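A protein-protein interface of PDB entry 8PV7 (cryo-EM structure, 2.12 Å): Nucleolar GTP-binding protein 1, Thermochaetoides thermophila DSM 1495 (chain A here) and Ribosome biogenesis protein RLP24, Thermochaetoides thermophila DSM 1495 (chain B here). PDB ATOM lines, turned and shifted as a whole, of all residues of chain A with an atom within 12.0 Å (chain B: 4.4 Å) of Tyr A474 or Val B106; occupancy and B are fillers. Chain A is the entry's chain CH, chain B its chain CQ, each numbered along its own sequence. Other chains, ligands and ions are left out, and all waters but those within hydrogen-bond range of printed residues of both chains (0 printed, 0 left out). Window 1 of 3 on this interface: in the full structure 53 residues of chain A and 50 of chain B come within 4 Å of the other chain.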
ATOM      1  N   LEU A 458      15.032  11.163 -20.885  1.00  0.00           N
ATOM      2  CA  LEU A 458      13.594  10.990 -21.063  1.00  0.00           C
ATOM      3  C   LEU A 458      13.002  10.093 -19.980  1.00  0.00           C
ATOM      4  O   LEU A 458      11.902  10.359 -19.481  1.00  0.00           O
ATOM      5  CB  LEU A 458      13.301  10.424 -22.450  1.00  0.00           C
ATOM      6  CG  LEU A 458      11.842  10.508 -22.904  1.00  0.00           C
ATOM      7  CD1 LEU A 458      11.296  11.913 -22.719  1.00  0.00           C
ATOM      8  CD2 LEU A 458      11.697  10.063 -24.347  1.00  0.00           C
ATOM      9  N   ALA A 460      14.235   9.772 -16.935  1.00  0.00           N
ATOM     10  CA  ALA A 460      14.235  10.598 -15.732  1.00  0.00           C
ATOM     11  C   ALA A 460      13.067  11.578 -15.734  1.00  0.00           C
ATOM     12  O   ALA A 460      12.443  11.816 -14.692  1.00  0.00           O
ATOM     13  CB  ALA A 460      15.561  11.344 -15.610  1.00  0.00           C
ATOM     14  N   LEU A 461      12.757  12.147 -16.902  1.00  0.00           N
ATOM     15  CA  LEU A 461      11.607  13.037 -17.025  1.00  0.00           C
ATOM     16  C   LEU A 461      10.305  12.307 -16.727  1.00  0.00           C
ATOM     17  O   LEU A 461       9.429  12.844 -16.040  1.00  0.00           O
ATOM     18  CB  LEU A 461      11.570  13.646 -18.426  1.00  0.00           C
ATOM     19  CG  LEU A 461      10.384  14.554 -18.752  1.00  0.00           C
ATOM     20  CD1 LEU A 461      10.374  15.762 -17.842  1.00  0.00           C
ATOM     21  CD2 LEU A 461      10.398  14.978 -20.208  1.00  0.00           C
ATOM     22  N   GLU A 462      10.163  11.078 -17.225  1.00  0.00           N
ATOM     23  CA  GLU A 462       8.940  10.318 -16.972  1.00  0.00           C
ATOM     24  C   GLU A 462       8.821   9.918 -15.503  1.00  0.00           C
ATOM     25  O   GLU A 462       7.715   9.907 -14.947  1.00  0.00           O
ATOM     26  CB  GLU A 462       8.884   9.088 -17.873  1.00  0.00           C
ATOM     27  CG  GLU A 462       8.811   9.406 -19.360  1.00  0.00           C
ATOM     28  CD  GLU A 462       7.422   9.799 -19.828  1.00  0.00           C
ATOM     29  OE1 GLU A 462       6.463   9.708 -19.034  1.00  0.00           O
ATOM     30  OE2 GLU A 462       7.288  10.194 -21.003  1.00  0.00           O
ATOM     31  N   GLU A 463       9.944   9.581 -14.865  1.00  0.00           N
ATOM     32  CA  GLU A 463       9.929   9.279 -13.435  1.00  0.00           C
ATOM     33  C   GLU A 463       9.526  10.500 -12.617  1.00  0.00           C
ATOM     34  O   GLU A 463       8.737  10.397 -11.670  1.00  0.00           O
ATOM     35  CB  GLU A 463      11.296   8.760 -12.989  1.00  0.00           C
ATOM     36  CG  GLU A 463      11.641   7.388 -13.530  1.00  0.00           C
ATOM     37  CD  GLU A 463      13.101   7.037 -13.333  1.00  0.00           C
ATOM     38  OE1 GLU A 463      13.829   7.843 -12.717  1.00  0.00           O
ATOM     39  OE2 GLU A 463      13.522   5.959 -13.800  1.00  0.00           O
ATOM     40  N   GLU A 464      10.055  11.671 -12.980  1.00  0.00           N
ATOM     41  CA  GLU A 464       9.649  12.905 -12.316  1.00  0.00           C
ATOM     42  C   GLU A 464       8.170  13.193 -12.544  1.00  0.00           C
ATOM     43  O   GLU A 464       7.473  13.661 -11.638  1.00  0.00           O
ATOM     44  CB  GLU A 464      10.511  14.064 -12.814  1.00  0.00           C
ATOM     45  CG  GLU A 464      10.170  15.413 -12.221  1.00  0.00           C
ATOM     46  CD  GLU A 464      10.936  16.534 -12.884  1.00  0.00           C
ATOM     47  OE1 GLU A 464      11.619  16.261 -13.889  1.00  0.00           O
ATOM     48  OE2 GLU A 464      10.859  17.682 -12.403  1.00  0.00           O
ATOM     49  N   GLU A 465       7.672  12.890 -13.745  1.00  0.00           N
ATOM     50  CA  GLU A 465       6.268  13.126 -14.063  1.00  0.00           C
ATOM     51  C   GLU A 465       5.347  12.247 -13.226  1.00  0.00           C
ATOM     52  O   GLU A 465       4.344  12.725 -12.681  1.00  0.00           O
ATOM     53  CB  GLU A 465       6.029  12.897 -15.555  1.00  0.00           C
ATOM     54  CG  GLU A 465       4.619  13.203 -16.029  1.00  0.00           C
ATOM     55  CD  GLU A 465       4.344  14.688 -16.190  1.00  0.00           C
ATOM     56  OE1 GLU A 465       5.264  15.505 -15.984  1.00  0.00           O
ATOM     57  OE2 GLU A 465       3.196  15.039 -16.534  1.00  0.00           O
ATOM     58  N   GLU A 466       5.671  10.958 -13.100  1.00  0.00           N
ATOM     59  CA  GLU A 466       4.812  10.078 -12.311  1.00  0.00           C
ATOM     60  C   GLU A 466       4.935  10.383 -10.821  1.00  0.00           C
ATOM     61  O   GLU A 466       3.962  10.245 -10.068  1.00  0.00           O
ATOM     62  CB  GLU A 466       5.113   8.605 -12.601  1.00  0.00           C
ATOM     63  CG  GLU A 466       6.556   8.193 -12.443  1.00  0.00           C
ATOM     64  CD  GLU A 466       6.835   7.531 -11.113  1.00  0.00           C
ATOM     65  OE1 GLU A 466       8.024   7.360 -10.770  1.00  0.00           O
ATOM     66  OE2 GLU A 466       5.868   7.182 -10.408  1.00  0.00           O
ATOM     67  N   ARG A 467       6.114  10.834 -10.379  1.00  0.00           N
ATOM     68  CA  ARG A 467       6.265  11.267  -8.993  1.00  0.00           C
ATOM     69  C   ARG A 467       5.400  12.488  -8.696  1.00  0.00           C
ATOM     70  O   ARG A 467       4.741  12.559  -7.652  1.00  0.00           O
ATOM     71  CB  ARG A 467       7.734  11.565  -8.701  1.00  0.00           C
ATOM     72  CG  ARG A 467       8.022  11.883  -7.252  1.00  0.00           C
ATOM     73  CD  ARG A 467       8.591  13.277  -7.105  1.00  0.00           C
ATOM     74  NE  ARG A 467       9.945  13.372  -7.632  1.00  0.00           N
ATOM     75  CZ  ARG A 467      10.538  14.508  -7.971  1.00  0.00           C
ATOM     76  NH1 ARG A 467       9.921  15.672  -7.852  1.00  0.00           N
ATOM     77  NH2 ARG A 467      11.780  14.476  -8.444  1.00  0.00           N
ATOM     78  N   LEU A 468       5.381  13.459  -9.615  1.00  0.00           N
ATOM     79  CA  LEU A 468       4.546  14.642  -9.428  1.00  0.00           C
ATOM     80  C   LEU A 468       3.065  14.292  -9.496  1.00  0.00           C
ATOM     81  O   LEU A 468       2.246  14.881  -8.779  1.00  0.00           O
ATOM     82  CB  LEU A 468       4.895  15.701 -10.474  1.00  0.00           C
ATOM     83  CG  LEU A 468       6.222  16.438 -10.303  1.00  0.00           C
ATOM     84  CD1 LEU A 468       6.460  17.369 -11.478  1.00  0.00           C
ATOM     85  CD2 LEU A 468       6.254  17.203  -8.997  1.00  0.00           C
ATOM     86  N   GLU A 469       2.703  13.334 -10.351  1.00  0.00           N
ATOM     87  CA  GLU A 469       1.311  12.903 -10.432  1.00  0.00           C
ATOM     88  C   GLU A 469       0.872  12.195  -9.156  1.00  0.00           C
ATOM     89  O   GLU A 469      -0.286  12.316  -8.739  1.00  0.00           O
ATOM     90  CB  GLU A 469       1.114  11.999 -11.645  1.00  0.00           C
ATOM     91  CG  GLU A 469      -0.186  12.242 -12.380  1.00  0.00           C
ATOM     92  CD  GLU A 469      -0.015  12.211 -13.882  1.00  0.00           C
ATOM     93  OE1 GLU A 469       1.114  11.948 -14.346  1.00  0.00           O
ATOM     94  OE2 GLU A 469      -1.007  12.452 -14.601  1.00  0.00           O
ATOM     95  N   LYS A 470       1.776  11.435  -8.529  1.00  0.00           N
ATOM     96  CA  LYS A 470       1.459  10.851  -7.229  1.00  0.00           C
ATOM     97  C   LYS A 470       1.356  11.920  -6.147  1.00  0.00           C
ATOM     98  O   LYS A 470       0.484  11.843  -5.275  1.00  0.00           O
ATOM     99  CB  LYS A 470       2.498   9.801  -6.843  1.00  0.00           C
ATOM    100  CG  LYS A 470       2.309   8.469  -7.537  1.00  0.00           C
ATOM    101  CD  LYS A 470       3.584   7.650  -7.529  1.00  0.00           C
ATOM    102  CE  LYS A 470       3.434   6.405  -8.385  1.00  0.00           C
ATOM    103  NZ  LYS A 470       4.739   5.724  -8.602  1.00  0.00           N
ATOM    104  N   GLU A 471       2.229  12.926  -6.187  1.00  0.00           N
ATOM    105  CA  GLU A 471       2.158  13.987  -5.187  1.00  0.00           C
ATOM    106  C   GLU A 471       1.031  14.977  -5.444  1.00  0.00           C
ATOM    107  O   GLU A 471       0.811  15.860  -4.609  1.00  0.00           O
ATOM    108  CB  GLU A 471       3.487  14.739  -5.105  1.00  0.00           C
ATOM    109  CG  GLU A 471       4.654  13.891  -4.642  1.00  0.00           C
ATOM    110  CD  GLU A 471       5.987  14.576  -4.862  1.00  0.00           C
ATOM    111  OE1 GLU A 471       6.034  15.554  -5.636  1.00  0.00           O
ATOM    112  OE2 GLU A 471       6.990  14.136  -4.260  1.00  0.00           O
ATOM    113  N   GLY A 472       0.324  14.872  -6.567  1.00  0.00           N
ATOM    114  CA  GLY A 472      -0.792  15.763  -6.809  1.00  0.00           C
ATOM    115  C   GLY A 472      -0.404  17.118  -7.343  1.00  0.00           C
ATOM    116  O   GLY A 472      -1.083  18.107  -7.055  1.00  0.00           O
ATOM    117  N   PHE A 473       0.687  17.190  -8.106  1.00  0.00           N
ATOM    118  CA  PHE A 473       1.125  18.456  -8.683  1.00  0.00           C
ATOM    119  C   PHE A 473       0.136  18.951  -9.731  1.00  0.00           C
ATOM    120  O   PHE A 473      -0.084  20.160  -9.865  1.00  0.00           O
ATOM    121  CB  PHE A 473       2.524  18.277  -9.275  1.00  0.00           C
ATOM    122  CG  PHE A 473       3.102  19.515  -9.898  1.00  0.00           C
ATOM    123  CD1 PHE A 473       3.013  19.730 -11.264  1.00  0.00           C
ATOM    124  CD2 PHE A 473       3.769  20.445  -9.120  1.00  0.00           C
ATOM    125  CE1 PHE A 473       3.554  20.860 -11.834  1.00  0.00           C
ATOM    126  CE2 PHE A 473       4.317  21.577  -9.689  1.00  0.00           C
ATOM    127  CZ  PHE A 473       4.208  21.783 -11.047  1.00  0.00           C
ATOM    128  N   TYR A 474      -0.480  18.033 -10.472  1.00  0.00           N
ATOM    129  CA  TYR A 474      -1.426  18.376 -11.523  1.00  0.00           C
ATOM    130  C   TYR A 474      -2.876  18.310 -11.064  1.00  0.00           C
ATOM    131  O   TYR A 474      -3.779  18.402 -11.901  1.00  0.00           O
ATOM    132  CB  TYR A 474      -1.233  17.459 -12.733  1.00  0.00           C
ATOM    133  CG  TYR A 474       0.158  17.482 -13.313  1.00  0.00           C
ATOM    134  CD1 TYR A 474       0.538  18.465 -14.218  1.00  0.00           C
ATOM    135  CD2 TYR A 474       1.092  16.518 -12.962  1.00  0.00           C
ATOM    136  CE1 TYR A 474       1.810  18.489 -14.750  1.00  0.00           C
ATOM    137  CE2 TYR A 474       2.365  16.534 -13.491  1.00  0.00           C
ATOM    138  CZ  TYR A 474       2.718  17.520 -14.384  1.00  0.00           C
ATOM    139  OH  TYR A 474       3.987  17.536 -14.911  1.00  0.00           O
ATOM    140  N   ASP A 475      -3.120  18.145  -9.767  1.00  0.00           N
ATOM    141  CA  ASP A 475      -4.480  18.014  -9.258  1.00  0.00           C
ATOM    142  C   ASP A 475      -5.170  19.371  -9.262  1.00  0.00           C
ATOM    143  O   ASP A 475      -4.630  20.352  -8.738  1.00  0.00           O
ATOM    144  CB  ASP A 475      -4.468  17.419  -7.852  1.00  0.00           C
ATOM    145  CG  ASP A 475      -4.191  15.931  -7.854  1.00  0.00           C
ATOM    146  OD1 ASP A 475      -3.786  15.401  -8.911  1.00  0.00           O
ATOM    147  OD2 ASP A 475      -4.382  15.289  -6.800  1.00  0.00           O
ATOM    148  N   GLU A 476      -6.364  19.423  -9.842  1.00  0.00           N
ATOM    149  CA  GLU A 476      -7.142  20.649  -9.940  1.00  0.00           C
ATOM    150  C   GLU A 476      -8.242  20.637  -8.888  1.00  0.00           C
ATOM    151  O   GLU A 476      -8.773  19.573  -8.552  1.00  0.00           O
ATOM    152  CB  GLU A 476      -7.747  20.801 -11.336  1.00  0.00           C
ATOM    153  CG  GLU A 476      -6.722  20.781 -12.458  1.00  0.00           C
ATOM    154  CD  GLU A 476      -7.345  21.003 -13.823  1.00  0.00           C
ATOM    155  OE1 GLU A 476      -8.575  21.207 -13.890  1.00  0.00           O
ATOM    156  OE2 GLU A 476      -6.604  20.972 -14.827  1.00  0.00           O
ATOM    157  N   ASP A 477      -8.578  21.815  -8.372  1.00  0.00           N
ATOM    158  CA  ASP A 477      -9.608  21.939  -7.349  1.00  0.00           C
ATOM    159  C   ASP A 477     -10.999  21.702  -7.930  1.00  0.00           C
ATOM    160  O   ASP A 477     -11.218  21.871  -9.129  1.00  0.00           O
ATOM    161  CB  ASP A 477      -9.543  23.318  -6.691  1.00  0.00           C
ATOM    162  CG  ASP A 477      -8.159  23.649  -6.172  1.00  0.00           C
ATOM    163  OD1 ASP A 477      -7.244  22.818  -6.346  1.00  0.00           O
ATOM    164  OD2 ASP A 477      -7.986  24.741  -5.591  1.00  0.00           O
ATOM    165  N   ARG B 102       1.657  21.171 -19.873  1.00  0.00           N
ATOM    166  CA  ARG B 102       0.950  20.917 -18.615  1.00  0.00           C
ATOM    167  C   ARG B 102       1.581  21.681 -17.451  1.00  0.00           C
ATOM    168  O   ARG B 102       0.882  22.318 -16.643  1.00  0.00           O
ATOM    169  CB  ARG B 102       0.932  19.420 -18.320  1.00  0.00           C
ATOM    170  CG  ARG B 102      -0.111  18.648 -19.097  1.00  0.00           C
ATOM    171  CD  ARG B 102      -0.858  17.684 -18.198  1.00  0.00           C
ATOM    172  NE  ARG B 102       0.039  16.724 -17.566  1.00  0.00           N
ATOM    173  CZ  ARG B 102      -0.332  15.857 -16.635  1.00  0.00           C
ATOM    174  NH1 ARG B 102      -1.580  15.802 -16.200  1.00  0.00           N
ATOM    175  NH2 ARG B 102       0.571  15.024 -16.128  1.00  0.00           N
ATOM    176  N   ARG B 103       2.913  21.648 -17.367  1.00  0.00           N
ATOM    177  CA  ARG B 103       3.593  22.330 -16.272  1.00  0.00           C
ATOM    178  C   ARG B 103       3.453  23.844 -16.381  1.00  0.00           C
ATOM    179  O   ARG B 103       3.368  24.540 -15.362  1.00  0.00           O
ATOM    180  CB  ARG B 103       5.061  21.918 -16.232  1.00  0.00           C
ATOM    181  CG  ARG B 103       5.249  20.453 -15.914  1.00  0.00           C
ATOM    182  CD  ARG B 103       6.702  20.113 -15.717  1.00  0.00           C
ATOM    183  NE  ARG B 103       6.880  18.720 -15.332  1.00  0.00           N
ATOM    184  CZ  ARG B 103       8.056  18.159 -15.091  1.00  0.00           C
ATOM    185  NH1 ARG B 103       9.180  18.849 -15.177  1.00  0.00           N
ATOM    186  NH2 ARG B 103       8.104  16.874 -14.757  1.00  0.00           N
ATOM    187  N   GLU B 104       3.400  24.369 -17.609  1.00  0.00           N
ATOM    188  CA  GLU B 104       3.204  25.802 -17.786  1.00  0.00           C
ATOM    189  C   GLU B 104       1.822  26.235 -17.319  1.00  0.00           C
ATOM    190  O   GLU B 104       1.670  27.308 -16.717  1.00  0.00           O
ATOM    191  CB  GLU B 104       3.419  26.183 -19.250  1.00  0.00           C
ATOM    192  CG  GLU B 104       3.775  27.641 -19.452  1.00  0.00           C
ATOM    193  CD  GLU B 104       2.557  28.534 -19.539  1.00  0.00           C
ATOM    194  OE1 GLU B 104       1.539  28.096 -20.112  1.00  0.00           O
ATOM    195  OE2 GLU B 104       2.613  29.670 -19.024  1.00  0.00           O
ATOM    196  N   ARG B 105       0.799  25.419 -17.595  1.00  0.00           N
ATOM    197  CA  ARG B 105      -0.541  25.755 -17.116  1.00  0.00           C
ATOM    198  C   ARG B 105      -0.598  25.758 -15.589  1.00  0.00           C
ATOM    199  O   ARG B 105      -1.226  26.642 -14.982  1.00  0.00           O
ATOM    200  CB  ARG B 105      -1.569  24.791 -17.705  1.00  0.00           C
ATOM    201  CG  ARG B 105      -2.950  24.914 -17.097  1.00  0.00           C
ATOM    202  CD  ARG B 105      -3.983  24.187 -17.925  1.00  0.00           C
ATOM    203  NE  ARG B 105      -4.513  25.031 -18.988  1.00  0.00           N
ATOM    204  CZ  ARG B 105      -5.637  25.727 -18.900  1.00  0.00           C
ATOM    205  NH1 ARG B 105      -6.395  25.684 -17.817  1.00  0.00           N
ATOM    206  NH2 ARG B 105      -6.014  26.482 -19.927  1.00  0.00           N
ATOM    207  N   VAL B 106       0.079  24.795 -14.953  1.00  0.00           N
ATOM    208  CA  VAL B 106       0.148  24.784 -13.487  1.00  0.00           C
ATOM    209  C   VAL B 106       0.851  26.037 -12.959  1.00  0.00           C
ATOM    210  O   VAL B 106       0.414  26.647 -11.969  1.00  0.00           O
ATOM    211  CB  VAL B 106       0.832  23.494 -12.999  1.00  0.00           C
ATOM    212  CG1 VAL B 106       1.008  23.509 -11.496  1.00  0.00           C
ATOM    213  CG2 VAL B 106       0.023  22.288 -13.417  1.00  0.00           C
ATOM    214  N   PHE B 107       1.939  26.445 -13.620  1.00  0.00           N
ATOM    215  CA  PHE B 107       2.677  27.647 -13.230  1.00  0.00           C
ATOM    216  C   PHE B 107       1.797  28.896 -13.310  1.00  0.00           C
ATOM    217  O   PHE B 107       1.805  29.739 -12.398  1.00  0.00           O
ATOM    218  CB  PHE B 107       3.905  27.778 -14.135  1.00  0.00           C
ATOM    219  CG  PHE B 107       4.788  28.952 -13.831  1.00  0.00           C
ATOM    220  CD1 PHE B 107       5.781  28.855 -12.875  1.00  0.00           C
ATOM    221  CD2 PHE B 107       4.658  30.137 -14.535  1.00  0.00           C
ATOM    222  CE1 PHE B 107       6.608  29.926 -12.605  1.00  0.00           C
ATOM    223  CE2 PHE B 107       5.477  31.210 -14.267  1.00  0.00           C
ATOM    224  CZ  PHE B 107       6.454  31.105 -13.303  1.00  0.00           C
ATOM    225  N   TYR B 108       1.015  29.018 -14.384  1.00  0.00           N
ATOM    226  CA  TYR B 108       0.140  30.178 -14.541  1.00  0.00           C
ATOM    227  C   TYR B 108      -0.958  30.206 -13.481  1.00  0.00           C
ATOM    228  O   TYR B 108      -1.290  31.273 -12.946  1.00  0.00           O
ATOM    229  CB  TYR B 108      -0.461  30.196 -15.943  1.00  0.00           C
ATOM    230  CG  TYR B 108      -1.227  31.459 -16.247  1.00  0.00           C
ATOM    231  CD1 TYR B 108      -0.569  32.633 -16.577  1.00  0.00           C
ATOM    232  CD2 TYR B 108      -2.609  31.478 -16.198  1.00  0.00           C
ATOM    233  CE1 TYR B 108      -1.268  33.791 -16.851  1.00  0.00           C
ATOM    234  CE2 TYR B 108      -3.316  32.627 -16.471  1.00  0.00           C
ATOM    235  CZ  TYR B 108      -2.642  33.780 -16.798  1.00  0.00           C
ATOM    236  OH  TYR B 108      -3.346  34.926 -17.069  1.00  0.00           O
ATOM    237  N   LYS B 109      -1.539  29.043 -13.167  1.00  0.00           N
ATOM    238  CA  LYS B 109      -2.558  29.007 -12.118  1.00  0.00           C
ATOM    239  C   LYS B 109      -1.979  29.382 -10.758  1.00  0.00           C
ATOM    240  O   LYS B 109      -2.645  30.061  -9.957  1.00  0.00           O
ATOM    241  CB  LYS B 109      -3.206  27.627 -12.062  1.00  0.00           C
ATOM    242  CG  LYS B 109      -4.267  27.415 -13.118  1.00  0.00           C
ATOM    243  CD  LYS B 109      -4.510  25.940 -13.359  1.00  0.00           C
ATOM    244  CE  LYS B 109      -5.993  25.637 -13.446  1.00  0.00           C
ATOM    245  NZ  LYS B 109      -6.752  26.276 -12.338  1.00  0.00           N
ATOM    246  N   LYS B 110      -0.739  28.964 -10.486  1.00  0.00           N
ATOM    247  CA  LYS B 110      -0.075  29.381  -9.256  1.00  0.00           C
ATOM    248  C   LYS B 110       0.138  30.889  -9.223  1.00  0.00           C
ATOM    249  O   LYS B 110       0.077  31.503  -8.153  1.00  0.00           O
ATOM    250  CB  LYS B 110       1.253  28.646  -9.097  1.00  0.00           C
ATOM    251  CG  LYS B 110       1.155  27.376  -8.279  1.00  0.00           C
ATOM    252  CD  LYS B 110       2.531  26.830  -7.941  1.00  0.00           C
ATOM    253  CE  LYS B 110       2.550  25.310  -7.969  1.00  0.00           C
ATOM    254  NZ  LYS B 110       1.181  24.729  -7.903  1.00  0.00           N
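The side-chain carboxylate (OE2) of Glu A465 is in salt-bridge range of the guanidinium group (NH2) of Arg B102 (2.7 Å).
The guanidinium group (NH2) of Arg B102 is in salt-bridge range of the side-chain carboxylate (OE2) of Glu A469 (3.4 Å).
The side-chain carboxylate (OE2) of Glu A464 is in salt-bridge range of the guanidinium group (NH1) of Arg B103 (3.4 Å).
NH2 of Arg B103 is in salt-bridge range of OE1 of Glu A465, at 3.4 Å.
The guanidinium group (NE) of Arg B103 is in hydrogen-bond range of the side-chain hydroxyl (OH) of Tyr A474 (3.2 Å).
OE1 of Glu A465 is in hydrogen-bond range of OH of Tyr A474 (2.6 Å).
The backbone NH (N) of Phe A473 is in hydrogen-bond range of the backbone carbonyl oxygen (O) of Leu A468 (2.9 Å).
Among the printed residues, merely in contact across the chains: Tyr A474 with Arg B102 (3.5 Å), Phe A473 with Val B106 (3.7 Å), Leu A468 with Arg B103 (3.7 Å), Tyr A474 with Val B106 (3.9 Å) and Leu A461 with Arg B103 (3.99 Å).
Of chain B, only Arg B102, Arg B103 and Val B106 come within 4 Å of Tyr A474.
No residue of chain A comes within 4 Å of Phe B107.
No residue of chain A comes within 4 Å of Lys B110.
Of the printed residues of chain B, Glu A469 touches Arg B102.
Of the printed residues of chain B, Phe A473 touches Val B106 (3.7 Å).
Printed residues of chain A within 4 Å of Arg B103: Leu A461, Glu A464, Glu A465, Leu A468 and Tyr A474.
Printed residues of chain B within 4 Å of Leu A461: Arg B103 (3.99 Å).
Of the printed residues of chain B, Glu A465 touches Arg B102 (2.7 Å) and Arg B103 (3.4 Å).
Asp A475 touches none of the printed residues of chain B.
Of the 9 printed residues of chain B, 3 touch a printed residue of chain A.
Hydrophobic or aromatic side chains of chain B within 4 Å of the printed part of chain A: Val B106.
Among the printed residues, 10 pairs touch across the chains.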
